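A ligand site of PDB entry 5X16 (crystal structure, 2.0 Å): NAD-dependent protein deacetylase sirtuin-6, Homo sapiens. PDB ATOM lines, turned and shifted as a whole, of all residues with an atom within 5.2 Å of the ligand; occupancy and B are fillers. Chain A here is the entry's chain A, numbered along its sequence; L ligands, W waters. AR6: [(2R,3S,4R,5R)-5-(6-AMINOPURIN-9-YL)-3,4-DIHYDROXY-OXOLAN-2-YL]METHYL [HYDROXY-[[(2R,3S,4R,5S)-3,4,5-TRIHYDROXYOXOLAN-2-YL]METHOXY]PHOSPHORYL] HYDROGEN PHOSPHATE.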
ATOM      1  N   GLU A  20      29.380  19.857  -6.737  1.00  0.00           N
ATOM      2  CA  GLU A  20      28.782  19.619  -8.056  1.00  0.00           C
ATOM      3  C   GLU A  20      29.390  20.525  -9.111  1.00  0.00           C
ATOM      4  O   GLU A  20      29.867  21.617  -8.786  1.00  0.00           O
ATOM      5  CB  GLU A  20      27.286  19.830  -8.016  1.00  0.00           C
ATOM      6  CG  GLU A  20      26.580  18.778  -7.184  1.00  0.00           C
ATOM      7  CD  GLU A  20      25.220  19.233  -6.706  1.00  0.00           C
ATOM      8  OE1 GLU A  20      25.163  20.231  -5.954  1.00  0.00           O
ATOM      9  OE2 GLU A  20      24.198  18.615  -7.082  1.00  0.00           O
ATOM     10  N   GLY A  50      22.777   4.827 -11.389  1.00  0.00           N
ATOM     11  CA  GLY A  50      22.834   4.940  -9.958  1.00  0.00           C
ATOM     12  C   GLY A  50      21.822   5.926  -9.401  1.00  0.00           C
ATOM     13  O   GLY A  50      20.869   6.345 -10.078  1.00  0.00           O
ATOM     14  N   ALA A  51      22.084   6.322  -8.166  1.00  0.00           N
ATOM     15  CA  ALA A  51      21.104   6.971  -7.329  1.00  0.00           C
ATOM     16  C   ALA A  51      20.773   8.351  -7.857  1.00  0.00           C
ATOM     17  O   ALA A  51      19.679   8.838  -7.606  1.00  0.00           O
ATOM     18  CB  ALA A  51      21.599   7.041  -5.896  1.00  0.00           C
ATOM     19  N   GLY A  52      21.656   8.946  -8.660  1.00  0.00           N
ATOM     20  CA  GLY A  52      21.396  10.262  -9.228  1.00  0.00           C
ATOM     21  C   GLY A  52      20.211  10.352 -10.188  1.00  0.00           C
ATOM     22  O   GLY A  52      19.693  11.429 -10.396  1.00  0.00           O
ATOM     23  N   THR A  55      16.944  11.117  -7.834  1.00  0.00           N
ATOM     24  CA  THR A  55      16.817  12.338  -7.029  1.00  0.00           C
ATOM     25  C   THR A  55      15.637  13.218  -7.442  1.00  0.00           C
ATOM     26  O   THR A  55      14.958  13.742  -6.553  1.00  0.00           O
ATOM     27  CB  THR A  55      18.113  13.181  -7.002  1.00  0.00           C
ATOM     28  OG1 THR A  55      18.580  13.424  -8.341  1.00  0.00           O
ATOM     29  CG2 THR A  55      19.184  12.445  -6.197  1.00  0.00           C
ATOM     30  N   ASP A  61      20.198  10.674  -2.905  1.00  0.00           N
ATOM     31  CA  ASP A  61      21.332   9.853  -3.259  1.00  0.00           C
ATOM     32  C   ASP A  61      22.146   9.499  -1.990  1.00  0.00           C
ATOM     33  O   ASP A  61      21.664   9.684  -0.877  1.00  0.00           O
ATOM     34  CB  ASP A  61      22.121  10.475  -4.416  1.00  0.00           C
ATOM     35  CG  ASP A  61      22.820  11.737  -4.050  1.00  0.00           C
ATOM     36  OD1 ASP A  61      22.960  12.072  -2.872  1.00  0.00           O
ATOM     37  OD2 ASP A  61      23.290  12.392  -4.990  1.00  0.00           O
ATOM     38  N   PHE A  62      23.348   8.935  -2.159  1.00  0.00           N
ATOM     39  CA  PHE A  62      24.174   8.472  -1.043  1.00  0.00           C
ATOM     40  C   PHE A  62      25.351   9.400  -0.733  1.00  0.00           C
ATOM     41  O   PHE A  62      25.665   9.627   0.447  1.00  0.00           O
ATOM     42  CB  PHE A  62      24.650   7.050  -1.304  1.00  0.00           C
ATOM     43  CG  PHE A  62      23.547   6.062  -1.376  1.00  0.00           C
ATOM     44  CD1 PHE A  62      22.986   5.552  -0.197  1.00  0.00           C
ATOM     45  CD2 PHE A  62      22.978   5.701  -2.593  1.00  0.00           C
ATOM     46  CE1 PHE A  62      21.940   4.652  -0.250  1.00  0.00           C
ATOM     47  CE2 PHE A  62      21.929   4.805  -2.654  1.00  0.00           C
ATOM     48  CZ  PHE A  62      21.404   4.283  -1.479  1.00  0.00           C
ATOM     49  N   ARG A  63      25.985   9.913  -1.779  1.00  0.00           N
ATOM     50  CA  ARG A  63      27.234  10.676  -1.642  1.00  0.00           C
ATOM     51  C   ARG A  63      27.196  12.081  -2.234  1.00  0.00           C
ATOM     52  O   ARG A  63      28.236  12.746  -2.314  1.00  0.00           O
ATOM     53  CB  ARG A  63      28.389   9.878  -2.267  1.00  0.00           C
ATOM     54  CG  ARG A  63      28.519   8.473  -1.711  1.00  0.00           C
ATOM     55  CD  ARG A  63      29.660   7.681  -2.352  1.00  0.00           C
ATOM     56  NE  ARG A  63      29.684   6.343  -1.779  1.00  0.00           N
ATOM     57  CZ  ARG A  63      28.863   5.331  -2.100  1.00  0.00           C
ATOM     58  NH1 ARG A  63      27.919   5.466  -3.042  1.00  0.00           N
ATOM     59  NH2 ARG A  63      28.982   4.167  -1.473  1.00  0.00           N
ATOM     60  N   GLY A  64      26.015  12.526  -2.642  1.00  0.00           N
ATOM     61  CA  GLY A  64      25.801  13.897  -3.078  1.00  0.00           C
ATOM     62  C   GLY A  64      25.797  14.828  -1.866  1.00  0.00           C
ATOM     63  O   GLY A  64      25.788  14.366  -0.727  1.00  0.00           O
ATOM     64  N   TRP A  69      24.772   8.907   3.050  1.00  0.00           N
ATOM     65  CA  TRP A  69      26.060   8.758   3.756  1.00  0.00           C
ATOM     66  C   TRP A  69      26.674  10.103   4.083  1.00  0.00           C
ATOM     67  O   TRP A  69      27.333  10.241   5.115  1.00  0.00           O
ATOM     68  CB  TRP A  69      27.091   7.910   2.976  1.00  0.00           C
ATOM     69  CG  TRP A  69      26.617   6.575   2.478  1.00  0.00           C
ATOM     70  CD1 TRP A  69      27.013   5.944   1.330  1.00  0.00           C
ATOM     71  CD2 TRP A  69      25.666   5.695   3.105  1.00  0.00           C
ATOM     72  NE1 TRP A  69      26.381   4.737   1.206  1.00  0.00           N
ATOM     73  CE2 TRP A  69      25.542   4.556   2.281  1.00  0.00           C
ATOM     74  CE3 TRP A  69      24.912   5.762   4.286  1.00  0.00           C
ATOM     75  CZ2 TRP A  69      24.683   3.504   2.575  1.00  0.00           C
ATOM     76  CZ3 TRP A  69      24.060   4.692   4.592  1.00  0.00           C
ATOM     77  CH2 TRP A  69      23.955   3.585   3.745  1.00  0.00           C
ATOM     78  N   GLN A 111      22.489  -0.067 -10.033  1.00  0.00           N
ATOM     79  CA  GLN A 111      22.819  -0.199  -8.604  1.00  0.00           C
ATOM     80  C   GLN A 111      21.674   0.236  -7.684  1.00  0.00           C
ATOM     81  O   GLN A 111      21.775   0.131  -6.470  1.00  0.00           O
ATOM     82  CB  GLN A 111      24.052   0.654  -8.301  1.00  0.00           C
ATOM     83  CG  GLN A 111      25.283   0.274  -9.110  1.00  0.00           C
ATOM     84  CD  GLN A 111      26.398   1.315  -9.061  1.00  0.00           C
ATOM     85  OE1 GLN A 111      26.644   2.030 -10.028  1.00  0.00           O
ATOM     86  NE2 GLN A 111      27.080   1.412  -7.929  1.00  0.00           N
ATOM     87  N   ASN A 112      20.561   0.718  -8.263  1.00  0.00           N
ATOM     88  CA  ASN A 112      19.455   1.221  -7.481  1.00  0.00           C
ATOM     89  C   ASN A 112      18.563   0.119  -6.916  1.00  0.00           C
ATOM     90  O   ASN A 112      18.165  -0.839  -7.631  1.00  0.00           O
ATOM     91  CB  ASN A 112      18.614   2.222  -8.279  1.00  0.00           C
ATOM     92  CG  ASN A 112      19.423   3.417  -8.717  1.00  0.00           C
ATOM     93  OD1 ASN A 112      20.542   3.653  -8.218  1.00  0.00           O
ATOM     94  ND2 ASN A 112      18.883   4.184  -9.623  1.00  0.00           N
ATOM     95  N   HIS A 131      22.384  -4.521  -6.728  1.00  0.00           N
ATOM     96  CA  HIS A 131      22.392  -4.346  -5.263  1.00  0.00           C
ATOM     97  C   HIS A 131      21.087  -4.728  -4.597  1.00  0.00           C
ATOM     98  O   HIS A 131      20.936  -4.590  -3.387  1.00  0.00           O
ATOM     99  CB  HIS A 131      22.743  -2.906  -4.921  1.00  0.00           C
ATOM    100  CG  HIS A 131      24.117  -2.514  -5.368  1.00  0.00           C
ATOM    101  ND1 HIS A 131      24.562  -1.209  -5.318  1.00  0.00           N
ATOM    102  CD2 HIS A 131      25.149  -3.253  -5.849  1.00  0.00           C
ATOM    103  CE1 HIS A 131      25.810  -1.166  -5.762  1.00  0.00           C
ATOM    104  NE2 HIS A 131      26.179  -2.383  -6.097  1.00  0.00           N
ATOM    105  N   TRP A 186      26.390  -4.571   3.389  1.00  0.00           N
ATOM    106  CA  TRP A 186      27.800  -4.272   3.115  1.00  0.00           C
ATOM    107  C   TRP A 186      28.646  -5.553   3.016  1.00  0.00           C
ATOM    108  O   TRP A 186      28.485  -6.470   3.820  1.00  0.00           O
ATOM    109  CB  TRP A 186      28.363  -3.308   4.161  1.00  0.00           C
ATOM    110  CG  TRP A 186      27.831  -1.883   4.045  1.00  0.00           C
ATOM    111  CD1 TRP A 186      26.882  -1.305   4.836  1.00  0.00           C
ATOM    112  CD2 TRP A 186      28.217  -0.891   3.081  1.00  0.00           C
ATOM    113  NE1 TRP A 186      26.653  -0.008   4.436  1.00  0.00           N
ATOM    114  CE2 TRP A 186      27.450   0.268   3.363  1.00  0.00           C
ATOM    115  CE3 TRP A 186      29.121  -0.868   2.022  1.00  0.00           C
ATOM    116  CZ2 TRP A 186      27.578   1.454   2.614  1.00  0.00           C
ATOM    117  CZ3 TRP A 186      29.256   0.325   1.264  1.00  0.00           C
ATOM    118  CH2 TRP A 186      28.479   1.456   1.568  1.00  0.00           C
ATOM    119  N   GLY A 212      24.207   9.220 -13.352  1.00  0.00           N
ATOM    120  CA  GLY A 212      23.947   9.455 -11.936  1.00  0.00           C
ATOM    121  C   GLY A 212      24.541   8.407 -10.993  1.00  0.00           C
ATOM    122  O   GLY A 212      23.858   7.938 -10.085  1.00  0.00           O
ATOM    123  N   THR A 213      25.777   8.001 -11.251  1.00  0.00           N
ATOM    124  CA  THR A 213      26.514   7.156 -10.321  1.00  0.00           C
ATOM    125  C   THR A 213      27.915   7.695 -10.155  1.00  0.00           C
ATOM    126  O   THR A 213      28.544   8.117 -11.131  1.00  0.00           O
ATOM    127  CB  THR A 213      26.558   5.661 -10.725  1.00  0.00           C
ATOM    128  OG1 THR A 213      27.501   4.966  -9.888  1.00  0.00           O
ATOM    129  CG2 THR A 213      26.927   5.462 -12.210  1.00  0.00           C
ATOM    130  N   SER A 214      28.400   7.715  -8.908  1.00  0.00           N
ATOM    131  CA  SER A 214      29.762   8.174  -8.646  1.00  0.00           C
ATOM    132  C   SER A 214      30.804   7.081  -8.908  1.00  0.00           C
ATOM    133  O   SER A 214      32.026   7.348  -8.814  1.00  0.00           O
ATOM    134  CB  SER A 214      29.898   8.714  -7.211  1.00  0.00           C
ATOM    135  OG  SER A 214      29.590   7.706  -6.264  1.00  0.00           O
ATOM    136  N   LEU A 215      30.343   5.852  -9.216  1.00  0.00           N
ATOM    137  CA  LEU A 215      31.180   4.734  -9.634  1.00  0.00           C
ATOM    138  C   LEU A 215      32.176   4.284  -8.579  1.00  0.00           C
ATOM    139  O   LEU A 215      33.229   3.742  -8.917  1.00  0.00           O
ATOM    140  CB  LEU A 215      31.896   5.022 -10.968  1.00  0.00           C
ATOM    141  CG  LEU A 215      30.997   5.301 -12.172  1.00  0.00           C
ATOM    142  CD1 LEU A 215      31.812   5.745 -13.358  1.00  0.00           C
ATOM    143  CD2 LEU A 215      30.185   4.067 -12.517  1.00  0.00           C
ATOM    144  N   GLN A 216      31.844   4.504  -7.313  1.00  0.00           N
ATOM    145  CA  GLN A 216      32.751   4.210  -6.201  1.00  0.00           C
ATOM    146  C   GLN A 216      32.676   2.788  -5.634  1.00  0.00           C
ATOM    147  O   GLN A 216      33.536   2.418  -4.861  1.00  0.00           O
ATOM    148  CB  GLN A 216      32.523   5.189  -5.055  1.00  0.00           C
ATOM    149  CG  GLN A 216      32.826   6.614  -5.437  1.00  0.00           C
ATOM    150  CD  GLN A 216      32.970   7.535  -4.258  1.00  0.00           C
ATOM    151  OE1 GLN A 216      33.721   7.251  -3.318  1.00  0.00           O
ATOM    152  NE2 GLN A 216      32.271   8.660  -4.289  1.00  0.00           N
ATOM    153  N   ILE A 217      31.615   2.050  -5.946  1.00  0.00           N
ATOM    154  CA  ILE A 217      31.461   0.686  -5.456  1.00  0.00           C
ATOM    155  C   ILE A 217      32.079  -0.278  -6.441  1.00  0.00           C
ATOM    156  O   ILE A 217      31.912  -0.129  -7.639  1.00  0.00           O
ATOM    157  CB  ILE A 217      29.957   0.299  -5.261  1.00  0.00           C
ATOM    158  CG1 ILE A 217      29.337   1.096  -4.095  1.00  0.00           C
ATOM    159  CG2 ILE A 217      29.776  -1.217  -5.050  1.00  0.00           C
ATOM    160  CD1 ILE A 217      30.000   0.903  -2.727  1.00  0.00           C
ATOM    161  N   VAL A 237      27.903  10.633 -17.177  1.00  0.00           N
ATOM    162  CA  VAL A 237      26.990  11.726 -16.995  1.00  0.00           C
ATOM    163  C   VAL A 237      26.755  11.814 -15.500  1.00  0.00           C
ATOM    164  O   VAL A 237      26.141  10.897 -14.912  1.00  0.00           O
ATOM    165  CB  VAL A 237      25.647  11.500 -17.719  1.00  0.00           C
ATOM    166  CG1 VAL A 237      24.723  12.696 -17.515  1.00  0.00           C
ATOM    167  CG2 VAL A 237      25.845  11.247 -19.197  1.00  0.00           C
ATOM    168  N   ASN A 238      27.246  12.879 -14.880  1.00  0.00           N
ATOM    169  CA  ASN A 238      27.162  13.038 -13.434  1.00  0.00           C
ATOM    170  C   ASN A 238      27.500  14.446 -13.002  1.00  0.00           C
ATOM    171  O   ASN A 238      28.374  15.083 -13.618  1.00  0.00           O
ATOM    172  CB  ASN A 238      28.164  12.101 -12.726  1.00  0.00           C
ATOM    173  CG  ASN A 238      27.683  11.658 -11.360  1.00  0.00           C
ATOM    174  OD1 ASN A 238      26.638  11.042 -11.266  1.00  0.00           O
ATOM    175  ND2 ASN A 238      28.425  11.964 -10.310  1.00  0.00           N
ATOM    176  N   LEU A 239      26.842  14.920 -11.936  1.00  0.00           N
ATOM    177  CA  LEU A 239      27.097  16.280 -11.425  1.00  0.00           C
ATOM    178  C   LEU A 239      28.408  16.366 -10.638  1.00  0.00           C
ATOM    179  O   LEU A 239      29.112  17.364 -10.734  1.00  0.00           O
ATOM    180  CB  LEU A 239      25.946  16.811 -10.569  1.00  0.00           C
ATOM    181  CG  LEU A 239      24.709  17.220 -11.386  1.00  0.00           C
ATOM    182  CD1 LEU A 239      23.526  17.395 -10.452  1.00  0.00           C
ATOM    183  CD2 LEU A 239      24.956  18.469 -12.226  1.00  0.00           C
ATOM    184  N   GLN A 240      28.722  15.360  -9.842  1.00  0.00           N
ATOM    185  CA  GLN A 240      29.977  15.321  -9.094  1.00  0.00           C
ATOM    186  C   GLN A 240      31.035  14.627  -9.940  1.00  0.00           C
ATOM    187  O   GLN A 240      30.691  13.889 -10.879  1.00  0.00           O
ATOM    188  CB  GLN A 240      29.810  14.519  -7.800  1.00  0.00           C
ATOM    189  CG  GLN A 240      29.063  15.185  -6.657  1.00  0.00           C
ATOM    190  CD  GLN A 240      28.958  14.320  -5.389  1.00  0.00           C
ATOM    191  OE1 GLN A 240      28.920  14.858  -4.256  1.00  0.00           O
ATOM    192  NE2 GLN A 240      28.911  13.002  -5.551  1.00  0.00           N
ATOM    193  N   PRO A 241      32.326  14.791  -9.558  1.00  0.00           N
ATOM    194  CA  PRO A 241      33.353  13.897 -10.083  1.00  0.00           C
ATOM    195  C   PRO A 241      32.990  12.435  -9.808  1.00  0.00           C
ATOM    196  O   PRO A 241      32.267  12.133  -8.838  1.00  0.00           O
ATOM    197  CB  PRO A 241      34.633  14.294  -9.312  1.00  0.00           C
ATOM    198  CG  PRO A 241      34.354  15.649  -8.744  1.00  0.00           C
ATOM    199  CD  PRO A 241      32.877  15.719  -8.540  1.00  0.00           C
ATOM    200  N   GLY A 254      25.866  17.693 -15.770  1.00  0.00           N
ATOM    201  CA  GLY A 254      24.577  18.386 -15.859  1.00  0.00           C
ATOM    202  C   GLY A 254      23.478  17.533 -15.249  1.00  0.00           C
ATOM    203  O   GLY A 254      23.733  16.401 -14.873  1.00  0.00           O
ATOM    204  N   TYR A 255      22.272  18.083 -15.179  1.00  0.00           N
ATOM    205  CA  TYR A 255      21.151  17.344 -14.630  1.00  0.00           C
ATOM    206  C   TYR A 255      20.837  16.227 -15.601  1.00  0.00           C
ATOM    207  O   TYR A 255      20.630  16.461 -16.802  1.00  0.00           O
ATOM    208  CB  TYR A 255      19.917  18.223 -14.463  1.00  0.00           C
ATOM    209  CG  TYR A 255      20.097  19.366 -13.479  1.00  0.00           C
ATOM    210  CD1 TYR A 255      20.137  19.133 -12.118  1.00  0.00           C
ATOM    211  CD2 TYR A 255      20.196  20.685 -13.920  1.00  0.00           C
ATOM    212  CE1 TYR A 255      20.305  20.163 -11.212  1.00  0.00           C
ATOM    213  CE2 TYR A 255      20.350  21.725 -13.017  1.00  0.00           C
ATOM    214  CZ  TYR A 255      20.393  21.451 -11.667  1.00  0.00           C
ATOM    215  OH  TYR A 255      20.568  22.460 -10.762  1.00  0.00           O
ATOM    216  N   VAL A 256      20.765  15.006 -15.070  1.00  0.00           N
ATOM    217  CA  VAL A 256      20.568  13.866 -15.886  1.00  0.00           C
ATOM    218  C   VAL A 256      19.221  13.960 -16.628  1.00  0.00           C
ATOM    219  O   VAL A 256      19.180  13.677 -17.805  1.00  0.00           O
ATOM    220  CB  VAL A 256      20.741  12.555 -15.084  1.00  0.00           C
ATOM    221  CG1 VAL A 256      19.633  12.340 -14.060  1.00  0.00           C
ATOM    222  CG2 VAL A 256      20.818  11.382 -16.036  1.00  0.00           C
ATOM    223  N   ASP A 257      18.164  14.440 -15.986  1.00  0.00           N
ATOM    224  CA  ASP A 257      16.923  14.692 -16.721  1.00  0.00           C
ATOM    225  C   ASP A 257      17.080  15.677 -17.905  1.00  0.00           C
ATOM    226  O   ASP A 257      16.432  15.476 -18.926  1.00  0.00           O
ATOM    227  CB  ASP A 257      15.793  15.174 -15.815  1.00  0.00           C
ATOM    228  CG  ASP A 257      15.156  14.042 -14.997  1.00  0.00           C
ATOM    229  OD1 ASP A 257      15.310  12.838 -15.314  1.00  0.00           O
ATOM    230  OD2 ASP A 257      14.473  14.376 -14.031  1.00  0.00           O
HETATM  231  N1  AR6 L   1      21.750  14.634 -12.295  1.00  0.00           N
HETATM  232  C2  AR6 L   1      23.034  14.216 -12.409  1.00  0.00           C
HETATM  233  N3  AR6 L   1      23.737  13.751 -11.389  1.00  0.00           N
HETATM  234  C4  AR6 L   1      23.140  13.642 -10.179  1.00  0.00           C
HETATM  235  C5  AR6 L   1      21.765  14.070  -9.965  1.00  0.00           C
HETATM  236  C6  AR6 L   1      21.071  14.603 -11.114  1.00  0.00           C
HETATM  237  N6  AR6 L   1      19.791  15.019 -10.956  1.00  0.00           N
HETATM  238  N7  AR6 L   1      21.436  13.876  -8.684  1.00  0.00           N
HETATM  239  C8  AR6 L   1      22.533  13.346  -8.113  1.00  0.00           C
HETATM  240  N9  AR6 L   1      23.539  13.237  -9.002  1.00  0.00           N
HETATM  241  PA  AR6 L   1      26.068   7.995  -5.247  1.00  0.00           P
HETATM  242  PB  AR6 L   1      25.580   5.431  -6.505  1.00  0.00           P
HETATM  243  C1' AR6 L   1      24.846  12.618  -8.787  1.00  0.00           C
HETATM  244  O1A AR6 L   1      27.428   7.507  -4.782  1.00  0.00           O
HETATM  245  O1B AR6 L   1      26.804   5.660  -7.355  1.00  0.00           O
HETATM  246  C1D AR6 L   1      25.572   2.905  -1.844  1.00  0.00           C
HETATM  247  O1D AR6 L   1      26.188   2.389  -0.677  1.00  0.00           O
HETATM  248  C2' AR6 L   1      25.605  12.931  -7.517  1.00  0.00           C
HETATM  249  O2' AR6 L   1      26.425  14.017  -7.887  1.00  0.00           O
HETATM  250  O2A AR6 L   1      25.246   8.828  -4.321  1.00  0.00           O
HETATM  251  O2B AR6 L   1      24.287   4.934  -7.093  1.00  0.00           O
HETATM  252  C2D AR6 L   1      24.362   2.095  -2.327  1.00  0.00           C
HETATM  253  O2D AR6 L   1      24.512   0.686  -2.160  1.00  0.00           O
HETATM  254  C3' AR6 L   1      26.320  11.607  -7.223  1.00  0.00           C
HETATM  255  O3' AR6 L   1      27.713  11.556  -7.581  1.00  0.00           O
HETATM  256  O3A AR6 L   1      25.139   6.745  -5.662  1.00  0.00           O
HETATM  257  C3D AR6 L   1      24.380   2.406  -3.813  1.00  0.00           C
HETATM  258  O3D AR6 L   1      23.666   1.428  -4.583  1.00  0.00           O
HETATM  259  C4' AR6 L   1      25.602  10.557  -8.076  1.00  0.00           C
HETATM  260  O4' AR6 L   1      24.527  11.221  -8.721  1.00  0.00           O
HETATM  261  C4D AR6 L   1      25.874   2.422  -4.093  1.00  0.00           C
HETATM  262  O4D AR6 L   1      26.510   2.950  -2.923  1.00  0.00           O
HETATM  263  C5' AR6 L   1      25.118   9.380  -7.251  1.00  0.00           C
HETATM  264  O5' AR6 L   1      26.259   8.800  -6.615  1.00  0.00           O
HETATM  265  C5D AR6 L   1      26.235   3.187  -5.353  1.00  0.00           C
HETATM  266  O5D AR6 L   1      25.913   4.555  -5.231  1.00  0.00           O
HETATM  267  O   HOH W   1      29.253   4.912  -6.213  1.00  0.00           O
HETATM  268  O   HOH W   2      22.963  15.074  -5.191  1.00  0.00           O
HETATM  269  O   HOH W   3      25.078  16.010  -6.685  1.00  0.00           O
HETATM  270  O   HOH W   4      17.726  15.075 -13.148  1.00  0.00           O
HETATM  271  O   HOH W   5      17.251  12.747 -11.083  1.00  0.00           O
HETATM  272  O   HOH W   6      20.915   1.518  -3.871  1.00  0.00           O
HETATM  273  O   HOH W   7      20.634  15.820  -6.413  1.00  0.00           O
HETATM  274  O   HOH W   8      22.097  -0.363  -1.606  1.00  0.00           O
HETATM  275  O   HOH W   9      22.342   3.336  -6.195  1.00  0.00           O
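OG1 of Thr 213 sits at hydrogen-bond distance from O1B of the ligand, at 2.7 Å. An oxygen (O2A) of the ligand lies within hydrogen-bond range of the backbone NH of Phe 62, 2.9 Å away. An oxygen (O1A) of the ligand is in salt-bridge range of the guanidinium group (NH1) of Arg 63, at 2.7 Å. O3D of the ligand is in hydrogen-bond range of ND1 of His 131 (2.9 Å). N of Gln 240 sits close to O2' of the ligand, 3.3 Å away. The backbone NH (N) of Ser 214 lies within hydrogen-bond range of an oxygen (O1B) of the ligand, 3.0 Å away. The backbone NH (N) of Arg 63 is in hydrogen-bond range of an oxygen (O2A) of the ligand. An oxygen (O1D) of the ligand is in hydrogen-bond range of the indole nitrogen (NE1) of Trp 69, at 3.0 Å. O3' of the ligand lies within hydrogen-bond range of ND2 of Asn 238 (2.8 Å). The side-chain hydroxyl (OG) of Ser 214 is in hydrogen-bond range of an oxygen (O1A) of the ligand. The backbone NH of Val 256 sits at hydrogen-bond distance from a nitrogen (N1) of the ligand (3.0 Å). An oxygen (O3D) of the ligand sits at hydrogen-bond distance from the backbone carbonyl oxygen (O) of Gln 111, 3.0 Å away. NE2 of Gln 240 sits at hydrogen-bond distance from O3' of the ligand. The backbone NH (N) of Leu 239 lies within hydrogen-bond range of a nitrogen (N3) of the ligand, 3.4 Å away. The backbone NH (N) of Ala 51 is in hydrogen-bond range of an oxygen (O2B) of the ligand (2.8 Å). OG1 of Thr 55 sits at hydrogen-bond distance from N7 of the ligand (2.9 Å).
The backbone NH (N) of Gly 52 is in hydrogen-bond range of the backbone carbonyl oxygen (O) of Gly 212 (2.8 Å). The backbone carbonyl oxygen of Val 237 is in hydrogen-bond range of the backbone NH of Gly 212, 3.0 Å away. The side-chain hydroxyl of Ser 214 is in hydrogen-bond range of the side-chain amide nitrogen of Gln 216. The backbone NH (N) of Ala 51 is in hydrogen-bond range of the backbone carbonyl oxygen (O) of Gly 212 (3.1 Å). O of Gln 240 sits at hydrogen-bond distance from ND2 of Asn 238. The side-chain hydroxyl of Thr 213 lies within hydrogen-bond range of the backbone NH of Leu 215 (3.1 Å). The backbone NH (N) of Trp 69 lies within hydrogen-bond range of the backbone carbonyl oxygen (O) of Phe 62 (2.8 Å). The side-chain hydroxyl (OG1) of Thr 213 sits at hydrogen-bond distance from the side-chain amide oxygen (OE1) of Gln 111 (3.1 Å).
N7 of the ligand lies close to O of Gly 52 (3.5 Å). CA of Gly 50 touches O2B of the ligand (3.2 Å). OD2 of Asp 61 touches C8 of the ligand, 3.4 Å away. Trp 186 touches the ligand (CH2 to O1D, 3.3 Å). Gly 212 touches the ligand. Ile 217 touches the ligand. O of Gly 254 touches C2 of the ligand (3.4 Å). Tyr 255 touches the ligand (CA to N1, 3.6 Å). Of the 29 residues printed, 21 come within 4 Å of the ligand.
Water W9 lies within hydrogen-bond range of O2B of the ligand (2.7 Å), OD1 of Asn 112 (2.7 Å) and O of Gln 111 (3.3 Å). Water W3 lies within hydrogen-bond range of an oxygen (O2') of the ligand and the side-chain carboxylate (OE2) of Glu 20. Water W6 lies within hydrogen-bond range of an oxygen (O3D) of the ligand (2.8 Å) and the backbone carbonyl oxygen of Gln 111 (3.1 Å). Water W4 bridges the backbone NH of Asp 257 and a nitrogen (N6) of the ligand. Water W5 lies within hydrogen-bond range of the backbone carbonyl oxygen (O) of Gly 52, the side-chain hydroxyl (OG1) of Thr 55 and a nitrogen (N6) of the ligand.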
